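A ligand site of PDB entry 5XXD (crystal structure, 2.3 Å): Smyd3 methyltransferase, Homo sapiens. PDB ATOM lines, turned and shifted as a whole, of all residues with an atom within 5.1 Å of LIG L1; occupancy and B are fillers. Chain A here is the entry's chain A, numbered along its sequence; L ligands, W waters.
Water W5 lies within hydrogen-bond range of O of Cys 256 (2.5 Å), O5 of LIG L1 (2.5 Å) and OD1 of Asn 130 (3.1 Å). Water W4 lies within hydrogen-bond range of an oxygen (O2) of LIG L1 (2.6 Å), the side-chain amide oxygen (OD1) of Asn 179 (2.8 Å) and the backbone NH (N) of Glu 128 (2.8 Å). Water W6 bridges a nitrogen (N5) of LIG L1 (2.9 Å) and the backbone carbonyl oxygen (O) of Glu 258 (3.3 Å). Water W1 lies within hydrogen-bond range of N1 of LIG L1, OE1 of Glu 128 and O of Arg 12.
ND2 of Asn 130 lies within hydrogen-bond range of O4 of LIG L1. An oxygen (O4) of LIG L1 lies within hydrogen-bond range of the backbone carbonyl oxygen (O) of Tyr 255 (2.6 Å). A nitrogen (N1) of LIG L1 sits at hydrogen-bond distance from the backbone carbonyl oxygen (O) of Arg 12, at 2.6 Å. The backbone NH (N) of Asn 14 lies within hydrogen-bond range of an oxygen (O1) of LIG L1 (2.8 Å). The backbone carbonyl oxygen of Asn 14 sits at hydrogen-bond distance from a nitrogen (N1) of LIG L1 (2.8 Å). The backbone NH of His 204 lies within hydrogen-bond range of a nitrogen (N3) of LIG L1, 2.9 Å away. A nitrogen (N4) of LIG L1 lies within hydrogen-bond range of the backbone carbonyl oxygen of His 204 (2.8 Å). OD1 of Asn 203 is in hydrogen-bond range of N1 of LIG L1, at 2.9 Å. An oxygen (O2) of LIG L1 is in hydrogen-bond range of the side-chain hydroxyl of Tyr 122, 3.0 Å away. The side-chain hydroxyl of Tyr 255 is in hydrogen-bond range of an oxygen (O2) of LG2 L2.
O of Asn 14 is in hydrogen-bond range of ND2 of Asn 203 (3.2 Å). The side-chain hydroxyl (OH) of Tyr 122 lies within hydrogen-bond range of the side-chain amide nitrogen (ND2) of Asn 14 (2.9 Å). The backbone NH (N) of Tyr 237 is in hydrogen-bond range of a ring nitrogen (ND1) of His 204, at 2.9 Å. The backbone carbonyl oxygen (O) of Asp 126 sits at hydrogen-bond distance from the side-chain hydroxyl (OH) of Tyr 122 (3.0 Å). The backbone carbonyl oxygen of Leu 202 sits at hydrogen-bond distance from the side-chain hydroxyl of Tyr 237, 2.6 Å away. The side-chain amide nitrogen (ND2) of Asn 179 sits at hydrogen-bond distance from the side-chain sulfur (SG) of Cys 178 (3.4 Å). The backbone carbonyl oxygen of Glu 128 lies within hydrogen-bond range of the side-chain amide nitrogen of Asn 179 (3.1 Å). The side-chain sulfur of Cys 178 lies within hydrogen-bond range of the backbone carbonyl oxygen of Glu 128, 3.1 Å away.
The side-chain amide oxygen of Asn 179 lies close to a sulfur (S1) of LIG L1, 3.5 Å away. O of Ser 200 lies close to S1 of LIG L1 (3.4 Å). A sulfur (S1) of LIG L1 lies close to the side-chain hydroxyl (OH) of Tyr 237 (3.7 Å). Merely in contact with LIG L1: Phe 257, Cys 178, Leu 202, Leu 201, Glu 128 and Gly 13. Hydrophobic or aromatic side chains within 4 Å of LIG L1: Tyr 122, His 204, Tyr 237, Tyr 255 and Phe 257. 16 residues have an atom within 4 Å of LIG L1: Arg 12, Gly 13, Asn 14, Tyr 122, Glu 128, Asn 130, Cys 178, Asn 179, Ser 200, Leu 201, Leu 202, Asn 203, His 204, Tyr 237, Tyr 255 and Phe 257.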
ATOM      1  N   ASN A  11     -15.197  -7.866  -2.265  1.00  0.00           N
ATOM      2  CA  ASN A  11     -15.618  -9.268  -2.264  1.00  0.00           C
ATOM      3  C   ASN A  11     -17.077  -9.464  -1.861  1.00  0.00           C
ATOM      4  O   ASN A  11     -17.445 -10.583  -1.485  1.00  0.00           O
ATOM      5  CB  ASN A  11     -14.709 -10.084  -1.328  1.00  0.00           C
ATOM      6  CG  ASN A  11     -14.643  -9.517   0.074  1.00  0.00           C
ATOM      7  OD1 ASN A  11     -15.472  -8.710   0.469  1.00  0.00           O
ATOM      8  ND2 ASN A  11     -13.635  -9.942   0.829  1.00  0.00           N
ATOM      9  N   ARG A  12     -17.904  -8.430  -1.937  1.00  0.00           N
ATOM     10  CA  ARG A  12     -19.300  -8.520  -1.512  1.00  0.00           C
ATOM     11  C   ARG A  12     -20.242  -7.971  -2.572  1.00  0.00           C
ATOM     12  O   ARG A  12     -21.337  -7.500  -2.257  1.00  0.00           O
ATOM     13  CB  ARG A  12     -19.511  -7.793  -0.183  1.00  0.00           C
ATOM     14  CG  ARG A  12     -19.010  -8.569   1.021  1.00  0.00           C
ATOM     15  CD  ARG A  12     -18.031  -7.764   1.847  1.00  0.00           C
ATOM     16  NE  ARG A  12     -18.625  -6.558   2.409  1.00  0.00           N
ATOM     17  CZ  ARG A  12     -18.715  -6.317   3.715  1.00  0.00           C
ATOM     18  NH1 ARG A  12     -18.244  -7.200   4.582  1.00  0.00           N
ATOM     19  NH2 ARG A  12     -19.263  -5.197   4.149  1.00  0.00           N
ATOM     20  N   GLY A  13     -19.837  -8.006  -3.836  1.00  0.00           N
ATOM     21  CA  GLY A  13     -20.660  -7.416  -4.876  1.00  0.00           C
ATOM     22  C   GLY A  13     -20.755  -5.919  -4.705  1.00  0.00           C
ATOM     23  O   GLY A  13     -19.783  -5.241  -4.377  1.00  0.00           O
ATOM     24  N   ASN A  14     -21.953  -5.384  -4.939  1.00  0.00           N
ATOM     25  CA  ASN A  14     -22.191  -3.954  -4.804  1.00  0.00           C
ATOM     26  C   ASN A  14     -22.580  -3.615  -3.372  1.00  0.00           C
ATOM     27  O   ASN A  14     -23.041  -4.460  -2.595  1.00  0.00           O
ATOM     28  CB  ASN A  14     -23.286  -3.506  -5.774  1.00  0.00           C
ATOM     29  CG  ASN A  14     -22.877  -3.653  -7.226  1.00  0.00           C
ATOM     30  OD1 ASN A  14     -21.722  -3.421  -7.578  1.00  0.00           O
ATOM     31  ND2 ASN A  14     -23.814  -4.060  -8.065  1.00  0.00           N
ATOM     32  N   GLY A  15     -22.400  -2.344  -3.019  1.00  0.00           N
ATOM     33  CA  GLY A  15     -22.728  -1.874  -1.689  1.00  0.00           C
ATOM     34  C   GLY A  15     -22.939  -0.373  -1.672  1.00  0.00           C
ATOM     35  O   GLY A  15     -22.842   0.300  -2.697  1.00  0.00           O
ATOM     36  N   TYR A 122     -30.578   1.741  -7.454  1.00  0.00           N
ATOM     37  CA  TYR A 122     -30.457   0.323  -7.747  1.00  0.00           C
ATOM     38  C   TYR A 122     -31.842  -0.158  -8.157  1.00  0.00           C
ATOM     39  O   TYR A 122     -32.818   0.083  -7.448  1.00  0.00           O
ATOM     40  CB  TYR A 122     -29.962  -0.453  -6.522  1.00  0.00           C
ATOM     41  CG  TYR A 122     -29.042  -1.633  -6.800  1.00  0.00           C
ATOM     42  CD1 TYR A 122     -27.979  -1.522  -7.683  1.00  0.00           C
ATOM     43  CD2 TYR A 122     -29.237  -2.832  -6.145  1.00  0.00           C
ATOM     44  CE1 TYR A 122     -27.131  -2.599  -7.914  1.00  0.00           C
ATOM     45  CE2 TYR A 122     -28.409  -3.918  -6.378  1.00  0.00           C
ATOM     46  CZ  TYR A 122     -27.357  -3.794  -7.261  1.00  0.00           C
ATOM     47  OH  TYR A 122     -26.535  -4.871  -7.477  1.00  0.00           O
ATOM     48  N   ASP A 126     -31.100  -4.869 -11.420  1.00  0.00           N
ATOM     49  CA  ASP A 126     -29.725  -4.944 -10.919  1.00  0.00           C
ATOM     50  C   ASP A 126     -29.572  -5.872  -9.728  1.00  0.00           C
ATOM     51  O   ASP A 126     -28.436  -6.192  -9.364  1.00  0.00           O
ATOM     52  CB  ASP A 126     -29.239  -3.552 -10.514  1.00  0.00           C
ATOM     53  CG  ASP A 126     -29.343  -2.539 -11.640  1.00  0.00           C
ATOM     54  OD1 ASP A 126     -28.872  -2.834 -12.754  1.00  0.00           O
ATOM     55  OD2 ASP A 126     -29.900  -1.451 -11.396  1.00  0.00           O
ATOM     56  N   LEU A 127     -30.663  -6.309  -9.101  1.00  0.00           N
ATOM     57  CA  LEU A 127     -30.594  -7.030  -7.843  1.00  0.00           C
ATOM     58  C   LEU A 127     -29.778  -8.318  -7.986  1.00  0.00           C
ATOM     59  O   LEU A 127     -29.795  -8.982  -9.022  1.00  0.00           O
ATOM     60  CB  LEU A 127     -31.990  -7.358  -7.328  1.00  0.00           C
ATOM     61  CG  LEU A 127     -32.891  -6.163  -7.015  1.00  0.00           C
ATOM     62  CD1 LEU A 127     -34.230  -6.618  -6.466  1.00  0.00           C
ATOM     63  CD2 LEU A 127     -32.199  -5.226  -6.041  1.00  0.00           C
ATOM     64  N   GLU A 128     -29.045  -8.644  -6.926  1.00  0.00           N
ATOM     65  CA  GLU A 128     -28.267  -9.870  -6.901  1.00  0.00           C
ATOM     66  C   GLU A 128     -29.186 -11.075  -6.855  1.00  0.00           C
ATOM     67  O   GLU A 128     -30.175 -11.110  -6.110  1.00  0.00           O
ATOM     68  CB  GLU A 128     -27.334  -9.880  -5.688  1.00  0.00           C
ATOM     69  CG  GLU A 128     -26.610 -11.196  -5.459  1.00  0.00           C
ATOM     70  CD  GLU A 128     -25.556 -11.466  -6.523  1.00  0.00           C
ATOM     71  OE1 GLU A 128     -24.565 -10.708  -6.574  1.00  0.00           O
ATOM     72  OE2 GLU A 128     -25.725 -12.435  -7.291  1.00  0.00           O
ATOM     73  N   ASN A 130     -27.597 -14.442  -6.924  1.00  0.00           N
ATOM     74  CA  ASN A 130     -26.799 -15.510  -6.318  1.00  0.00           C
ATOM     75  C   ASN A 130     -27.064 -16.852  -6.975  1.00  0.00           C
ATOM     76  O   ASN A 130     -27.034 -17.898  -6.317  1.00  0.00           O
ATOM     77  CB  ASN A 130     -27.041 -15.594  -4.804  1.00  0.00           C
ATOM     78  CG  ASN A 130     -26.286 -14.545  -4.030  1.00  0.00           C
ATOM     79  OD1 ASN A 130     -25.160 -14.201  -4.372  1.00  0.00           O
ATOM     80  ND2 ASN A 130     -26.910 -14.015  -2.987  1.00  0.00           N
ATOM     81  N   CYS A 178     -33.171 -13.074  -1.589  1.00  0.00           N
ATOM     82  CA  CYS A 178     -32.044 -12.425  -0.933  1.00  0.00           C
ATOM     83  C   CYS A 178     -32.128 -10.905  -0.954  1.00  0.00           C
ATOM     84  O   CYS A 178     -31.132 -10.245  -0.630  1.00  0.00           O
ATOM     85  CB  CYS A 178     -30.734 -12.893  -1.572  1.00  0.00           C
ATOM     86  SG  CYS A 178     -30.363 -12.152  -3.168  1.00  0.00           S
ATOM     87  N   ASN A 179     -33.275 -10.330  -1.313  1.00  0.00           N
ATOM     88  CA  ASN A 179     -33.457  -8.889  -1.250  1.00  0.00           C
ATOM     89  C   ASN A 179     -34.761  -8.470  -0.593  1.00  0.00           C
ATOM     90  O   ASN A 179     -35.020  -7.261  -0.495  1.00  0.00           O
ATOM     91  CB  ASN A 179     -33.370  -8.266  -2.649  1.00  0.00           C
ATOM     92  CG  ASN A 179     -31.985  -8.354  -3.241  1.00  0.00           C
ATOM     93  OD1 ASN A 179     -31.078  -7.612  -2.852  1.00  0.00           O
ATOM     94  ND2 ASN A 179     -31.790  -9.274  -4.186  1.00  0.00           N
ATOM     95  N   SER A 200     -31.590  -2.260  -1.068  1.00  0.00           N
ATOM     96  CA  SER A 200     -30.992  -3.589  -1.218  1.00  0.00           C
ATOM     97  C   SER A 200     -29.515  -3.537  -1.566  1.00  0.00           C
ATOM     98  O   SER A 200     -28.922  -4.604  -1.761  1.00  0.00           O
ATOM     99  CB  SER A 200     -31.756  -4.387  -2.274  1.00  0.00           C
ATOM    100  OG  SER A 200     -33.071  -4.682  -1.847  1.00  0.00           O
ATOM    101  N   LEU A 201     -28.911  -2.355  -1.676  1.00  0.00           N
ATOM    102  CA  LEU A 201     -27.466  -2.269  -1.838  1.00  0.00           C
ATOM    103  C   LEU A 201     -26.724  -2.511  -0.533  1.00  0.00           C
ATOM    104  O   LEU A 201     -25.535  -2.849  -0.576  1.00  0.00           O
ATOM    105  CB  LEU A 201     -27.073  -0.904  -2.409  1.00  0.00           C
ATOM    106  CG  LEU A 201     -27.196  -0.721  -3.918  1.00  0.00           C
ATOM    107  CD1 LEU A 201     -27.193   0.762  -4.286  1.00  0.00           C
ATOM    108  CD2 LEU A 201     -26.074  -1.452  -4.628  1.00  0.00           C
ATOM    109  N   LEU A 202     -27.386  -2.349   0.601  1.00  0.00           N
ATOM    110  CA  LEU A 202     -26.730  -2.459   1.896  1.00  0.00           C
ATOM    111  C   LEU A 202     -26.322  -3.901   2.169  1.00  0.00           C
ATOM    112  O   LEU A 202     -27.166  -4.806   2.176  1.00  0.00           O
ATOM    113  CB  LEU A 202     -27.649  -1.946   3.000  1.00  0.00           C
ATOM    114  CG  LEU A 202     -27.921  -0.435   2.977  1.00  0.00           C
ATOM    115  CD1 LEU A 202     -29.308  -0.135   3.517  1.00  0.00           C
ATOM    116  CD2 LEU A 202     -26.875   0.291   3.802  1.00  0.00           C
ATOM    117  N   ASN A 203     -25.026  -4.126   2.389  1.00  0.00           N
ATOM    118  CA  ASN A 203     -24.540  -5.436   2.759  1.00  0.00           C
ATOM    119  C   ASN A 203     -24.741  -5.658   4.259  1.00  0.00           C
ATOM    120  O   ASN A 203     -24.972  -4.735   5.031  1.00  0.00           O
ATOM    121  CB  ASN A 203     -23.070  -5.587   2.393  1.00  0.00           C
ATOM    122  CG  ASN A 203     -22.868  -5.826   0.907  1.00  0.00           C
ATOM    123  OD1 ASN A 203     -23.600  -6.602   0.286  1.00  0.00           O
ATOM    124  ND2 ASN A 203     -21.884  -5.156   0.324  1.00  0.00           N
ATOM    125  N   HIS A 204     -24.637  -6.931   4.663  1.00  0.00           N
ATOM    126  CA  HIS A 204     -24.942  -7.328   6.023  1.00  0.00           C
ATOM    127  C   HIS A 204     -23.721  -7.198   6.930  1.00  0.00           C
ATOM    128  O   HIS A 204     -22.574  -7.355   6.488  1.00  0.00           O
ATOM    129  CB  HIS A 204     -25.453  -8.770   6.075  1.00  0.00           C
ATOM    130  CG  HIS A 204     -25.376  -9.396   7.426  1.00  0.00           C
ATOM    131  ND1 HIS A 204     -26.374  -9.256   8.368  1.00  0.00           N
ATOM    132  CD2 HIS A 204     -24.423 -10.157   8.006  1.00  0.00           C
ATOM    133  CE1 HIS A 204     -26.044  -9.902   9.470  1.00  0.00           C
ATOM    134  NE2 HIS A 204     -24.859 -10.458   9.275  1.00  0.00           N
ATOM    135  N   SER A 205     -23.981  -6.926   8.206  1.00  0.00           N
ATOM    136  CA  SER A 205     -22.968  -7.014   9.251  1.00  0.00           C
ATOM    137  C   SER A 205     -23.654  -7.400  10.552  1.00  0.00           C
ATOM    138  O   SER A 205     -24.731  -6.884  10.870  1.00  0.00           O
ATOM    139  CB  SER A 205     -22.197  -5.699   9.415  1.00  0.00           C
ATOM    140  OG  SER A 205     -21.438  -5.704  10.612  1.00  0.00           O
ATOM    141  N   TYR A 237     -29.037  -8.071   8.709  1.00  0.00           N
ATOM    142  CA  TYR A 237     -30.154  -8.750   8.062  1.00  0.00           C
ATOM    143  C   TYR A 237     -31.017  -9.518   9.049  1.00  0.00           C
ATOM    144  O   TYR A 237     -32.179  -9.805   8.739  1.00  0.00           O
ATOM    145  CB  TYR A 237     -29.651  -9.723   6.992  1.00  0.00           C
ATOM    146  CG  TYR A 237     -29.019  -9.097   5.762  1.00  0.00           C
ATOM    147  CD1 TYR A 237     -28.876  -7.716   5.649  1.00  0.00           C
ATOM    148  CD2 TYR A 237     -28.563  -9.890   4.716  1.00  0.00           C
ATOM    149  CE1 TYR A 237     -28.288  -7.153   4.525  1.00  0.00           C
ATOM    150  CE2 TYR A 237     -27.976  -9.337   3.597  1.00  0.00           C
ATOM    151  CZ  TYR A 237     -27.841  -7.963   3.510  1.00  0.00           C
ATOM    152  OH  TYR A 237     -27.263  -7.409   2.388  1.00  0.00           O
ATOM    153  N   TYR A 255     -28.962 -16.089   1.876  1.00  0.00           N
ATOM    154  CA  TYR A 255     -28.150 -15.049   1.257  1.00  0.00           C
ATOM    155  C   TYR A 255     -26.869 -15.549   0.614  1.00  0.00           C
ATOM    156  O   TYR A 255     -26.196 -14.761  -0.065  1.00  0.00           O
ATOM    157  CB  TYR A 255     -27.822 -13.961   2.291  1.00  0.00           C
ATOM    158  CG  TYR A 255     -29.062 -13.302   2.856  1.00  0.00           C
ATOM    159  CD1 TYR A 255     -29.795 -12.388   2.107  1.00  0.00           C
ATOM    160  CD2 TYR A 255     -29.522 -13.617   4.135  1.00  0.00           C
ATOM    161  CE1 TYR A 255     -30.929 -11.797   2.616  1.00  0.00           C
ATOM    162  CE2 TYR A 255     -30.659 -13.021   4.652  1.00  0.00           C
ATOM    163  CZ  TYR A 255     -31.363 -12.112   3.881  1.00  0.00           C
ATOM    164  OH  TYR A 255     -32.497 -11.521   4.390  1.00  0.00           O
ATOM    165  N   CYS A 256     -26.506 -16.821   0.809  1.00  0.00           N
ATOM    166  CA  CYS A 256     -25.411 -17.468   0.076  1.00  0.00           C
ATOM    167  C   CYS A 256     -24.069 -16.769   0.307  1.00  0.00           C
ATOM    168  O   CYS A 256     -23.343 -16.458  -0.632  1.00  0.00           O
ATOM    169  CB  CYS A 256     -25.729 -17.535  -1.417  1.00  0.00           C
ATOM    170  SG  CYS A 256     -27.178 -18.539  -1.861  1.00  0.00           S
ATOM    171  N   PHE A 257     -23.735 -16.538   1.578  1.00  0.00           N
ATOM    172  CA  PHE A 257     -22.398 -16.058   1.910  1.00  0.00           C
ATOM    173  C   PHE A 257     -22.040 -16.501   3.315  1.00  0.00           C
ATOM    174  O   PHE A 257     -22.915 -16.730   4.154  1.00  0.00           O
ATOM    175  CB  PHE A 257     -22.275 -14.534   1.780  1.00  0.00           C
ATOM    176  CG  PHE A 257     -22.932 -13.769   2.891  1.00  0.00           C
ATOM    177  CD1 PHE A 257     -22.188 -13.345   3.990  1.00  0.00           C
ATOM    178  CD2 PHE A 257     -24.266 -13.430   2.833  1.00  0.00           C
ATOM    179  CE1 PHE A 257     -22.780 -12.628   5.007  1.00  0.00           C
ATOM    180  CE2 PHE A 257     -24.871 -12.708   3.855  1.00  0.00           C
ATOM    181  CZ  PHE A 257     -24.113 -12.302   4.945  1.00  0.00           C
ATOM    182  N   GLU A 258     -20.745 -16.621   3.560  1.00  0.00           N
ATOM    183  CA  GLU A 258     -20.204 -16.921   4.874  1.00  0.00           C
ATOM    184  C   GLU A 258     -19.695 -15.629   5.503  1.00  0.00           C
ATOM    185  O   GLU A 258     -18.884 -14.916   4.893  1.00  0.00           O
ATOM    186  CB  GLU A 258     -19.070 -17.948   4.790  1.00  0.00           C
ATOM    187  CG  GLU A 258     -19.231 -18.952   3.658  1.00  0.00           C
ATOM    188  CD  GLU A 258     -20.270 -20.009   3.950  1.00  0.00           C
ATOM    189  OE1 GLU A 258     -20.643 -20.156   5.139  1.00  0.00           O
ATOM    190  OE2 GLU A 258     -20.707 -20.692   3.004  1.00  0.00           O
HETATM  191  N1  LIG L   1     -23.945  -7.137  -2.520  1.00  0.00           N
HETATM  192  C1  LIG L   1     -25.349  -7.021  -2.910  1.00  0.00           C
HETATM  193  C2  LIG L   1     -25.484  -6.608  -4.376  1.00  0.00           C
HETATM  194  O1  LIG L   1     -24.491  -6.464  -5.086  1.00  0.00           O
HETATM  195  O2  LIG L   1     -26.587  -6.415  -4.884  1.00  0.00           O
HETATM  196  C3  LIG L   1     -26.069  -6.031  -2.013  1.00  0.00           C
HETATM  197  C4  LIG L   1     -26.694  -6.651  -0.772  1.00  0.00           C
HETATM  198  S1  LIG L   1     -28.001  -7.838  -1.179  1.00  0.00           S
HETATM  199  C5  LIG L   1     -29.342  -7.273  -0.111  1.00  0.00           C
HETATM  200  C6  LIG L   1     -27.467  -9.298  -0.243  1.00  0.00           C
HETATM  201  C7  LIG L   1     -26.396 -10.111  -0.949  1.00  0.00           C
HETATM  202  O3  LIG L   1     -25.137  -9.455  -0.843  1.00  0.00           O
HETATM  203  C8  LIG L   1     -26.238 -11.487  -0.318  1.00  0.00           C
HETATM  204  O4  LIG L   1     -26.943 -12.457  -1.060  1.00  0.00           O
HETATM  205  C9  LIG L   1     -24.755 -11.743  -0.364  1.00  0.00           C
HETATM  206  O5  LIG L   1     -24.444 -12.412  -1.559  1.00  0.00           O
HETATM  207  C10 LIG L   1     -24.134 -10.366  -0.424  1.00  0.00           C
HETATM  208  N2  LIG L   1     -23.684  -9.963   0.921  1.00  0.00           N
HETATM  209  C11 LIG L   1     -24.370  -9.140   1.770  1.00  0.00           C
HETATM  210  N3  LIG L   1     -23.659  -9.001   2.902  1.00  0.00           N
HETATM  211  C12 LIG L   1     -22.528  -9.721   2.794  1.00  0.00           C
HETATM  212  C13 LIG L   1     -21.460  -9.923   3.660  1.00  0.00           C
HETATM  213  N4  LIG L   1     -21.454  -9.340   4.861  1.00  0.00           N
HETATM  214  N5  LIG L   1     -20.413 -10.743   3.277  1.00  0.00           N
HETATM  215  C14 LIG L   1     -20.436 -11.346   2.033  1.00  0.00           C
HETATM  216  N6  LIG L   1     -21.496 -11.129   1.175  1.00  0.00           N
HETATM  217  C15 LIG L   1     -22.530 -10.337   1.553  1.00  0.00           C
HETATM  218  C1  LG2 L   2     -37.955  -5.962   9.902  1.00  0.00           C
HETATM  219  C2  LG2 L   2     -36.834  -5.574   9.192  1.00  0.00           C
HETATM  220  C3  LG2 L   2     -35.638  -5.191   9.798  1.00  0.00           C
HETATM  221  C4  LG2 L   2     -35.536  -5.621  11.116  1.00  0.00           C
HETATM  222  C5  LG2 L   2     -36.619  -6.084  11.846  1.00  0.00           C
HETATM  223  C6  LG2 L   2     -37.854  -6.258  11.238  1.00  0.00           C
HETATM  224  C7  LG2 L   2     -37.502  -6.862  13.839  1.00  0.00           C
HETATM  225  C8  LG2 L   2     -38.782  -6.939  13.291  1.00  0.00           C
HETATM  226  C9  LG2 L   2     -38.973  -6.705  11.946  1.00  0.00           C
HETATM  227  C10 LG2 L   2     -37.412  -7.022  15.189  1.00  0.00           C
HETATM  228  C11 LG2 L   2     -38.370  -7.912  16.007  1.00  0.00           C
HETATM  229  C12 LG2 L   2     -39.711  -7.237  15.678  1.00  0.00           C
HETATM  230  C13 LG2 L   2     -39.757  -7.449  14.112  1.00  0.00           C
HETATM  231  C14 LG2 L   2     -34.364  -4.981   9.284  1.00  0.00           C
HETATM  232  C15 LG2 L   2     -34.475  -6.963   7.831  1.00  0.00           C
HETATM  233  C16 LG2 L   2     -34.622  -7.218   6.351  1.00  0.00           C
HETATM  234  C17 LG2 L   2     -32.774  -5.648   6.013  1.00  0.00           C
HETATM  235  C18 LG2 L   2     -32.678  -5.438   7.525  1.00  0.00           C
HETATM  236  C19 LG2 L   2     -32.831  -7.763   4.730  1.00  0.00           C
HETATM  237  C20 LG2 L   2     -31.321  -8.326   3.067  1.00  0.00           C
HETATM  238  C21 LG2 L   2     -32.215  -7.861   1.905  1.00  0.00           C
HETATM  239  N1  LG2 L   2     -36.465  -6.371  13.148  1.00  0.00           N
HETATM  240  N2  LG2 L   2     -34.018  -5.585   8.136  1.00  0.00           N
HETATM  241  N3  LG2 L   2     -33.293  -7.003   5.733  1.00  0.00           N
HETATM  242  O1  LG2 L   2     -33.877  -3.863   9.497  1.00  0.00           O
HETATM  243  O2  LG2 L   2     -33.362  -8.851   4.520  1.00  0.00           O
HETATM  244  O3  LG2 L   2     -31.598  -7.497   4.205  1.00  0.00           O
HETATM  245  O   HOH W   1     -23.358  -9.876  -3.668  1.00  0.00           O
HETATM  246  O   HOH W   2     -20.863 -12.424  -1.407  1.00  0.00           O
HETATM  247  O   HOH W   3     -19.281  -9.891   6.908  1.00  0.00           O
HETATM  248  O   HOH W   4     -29.061  -7.036  -4.646  1.00  0.00           O
HETATM  249  O   HOH W   5     -23.090 -14.496  -2.111  1.00  0.00           O
HETATM  250  O   HOH W   6     -18.069 -11.777   4.589  1.00  0.00           O
HETATM  251  O   HOH W   7     -29.800  -4.653   2.111  1.00  0.00           O
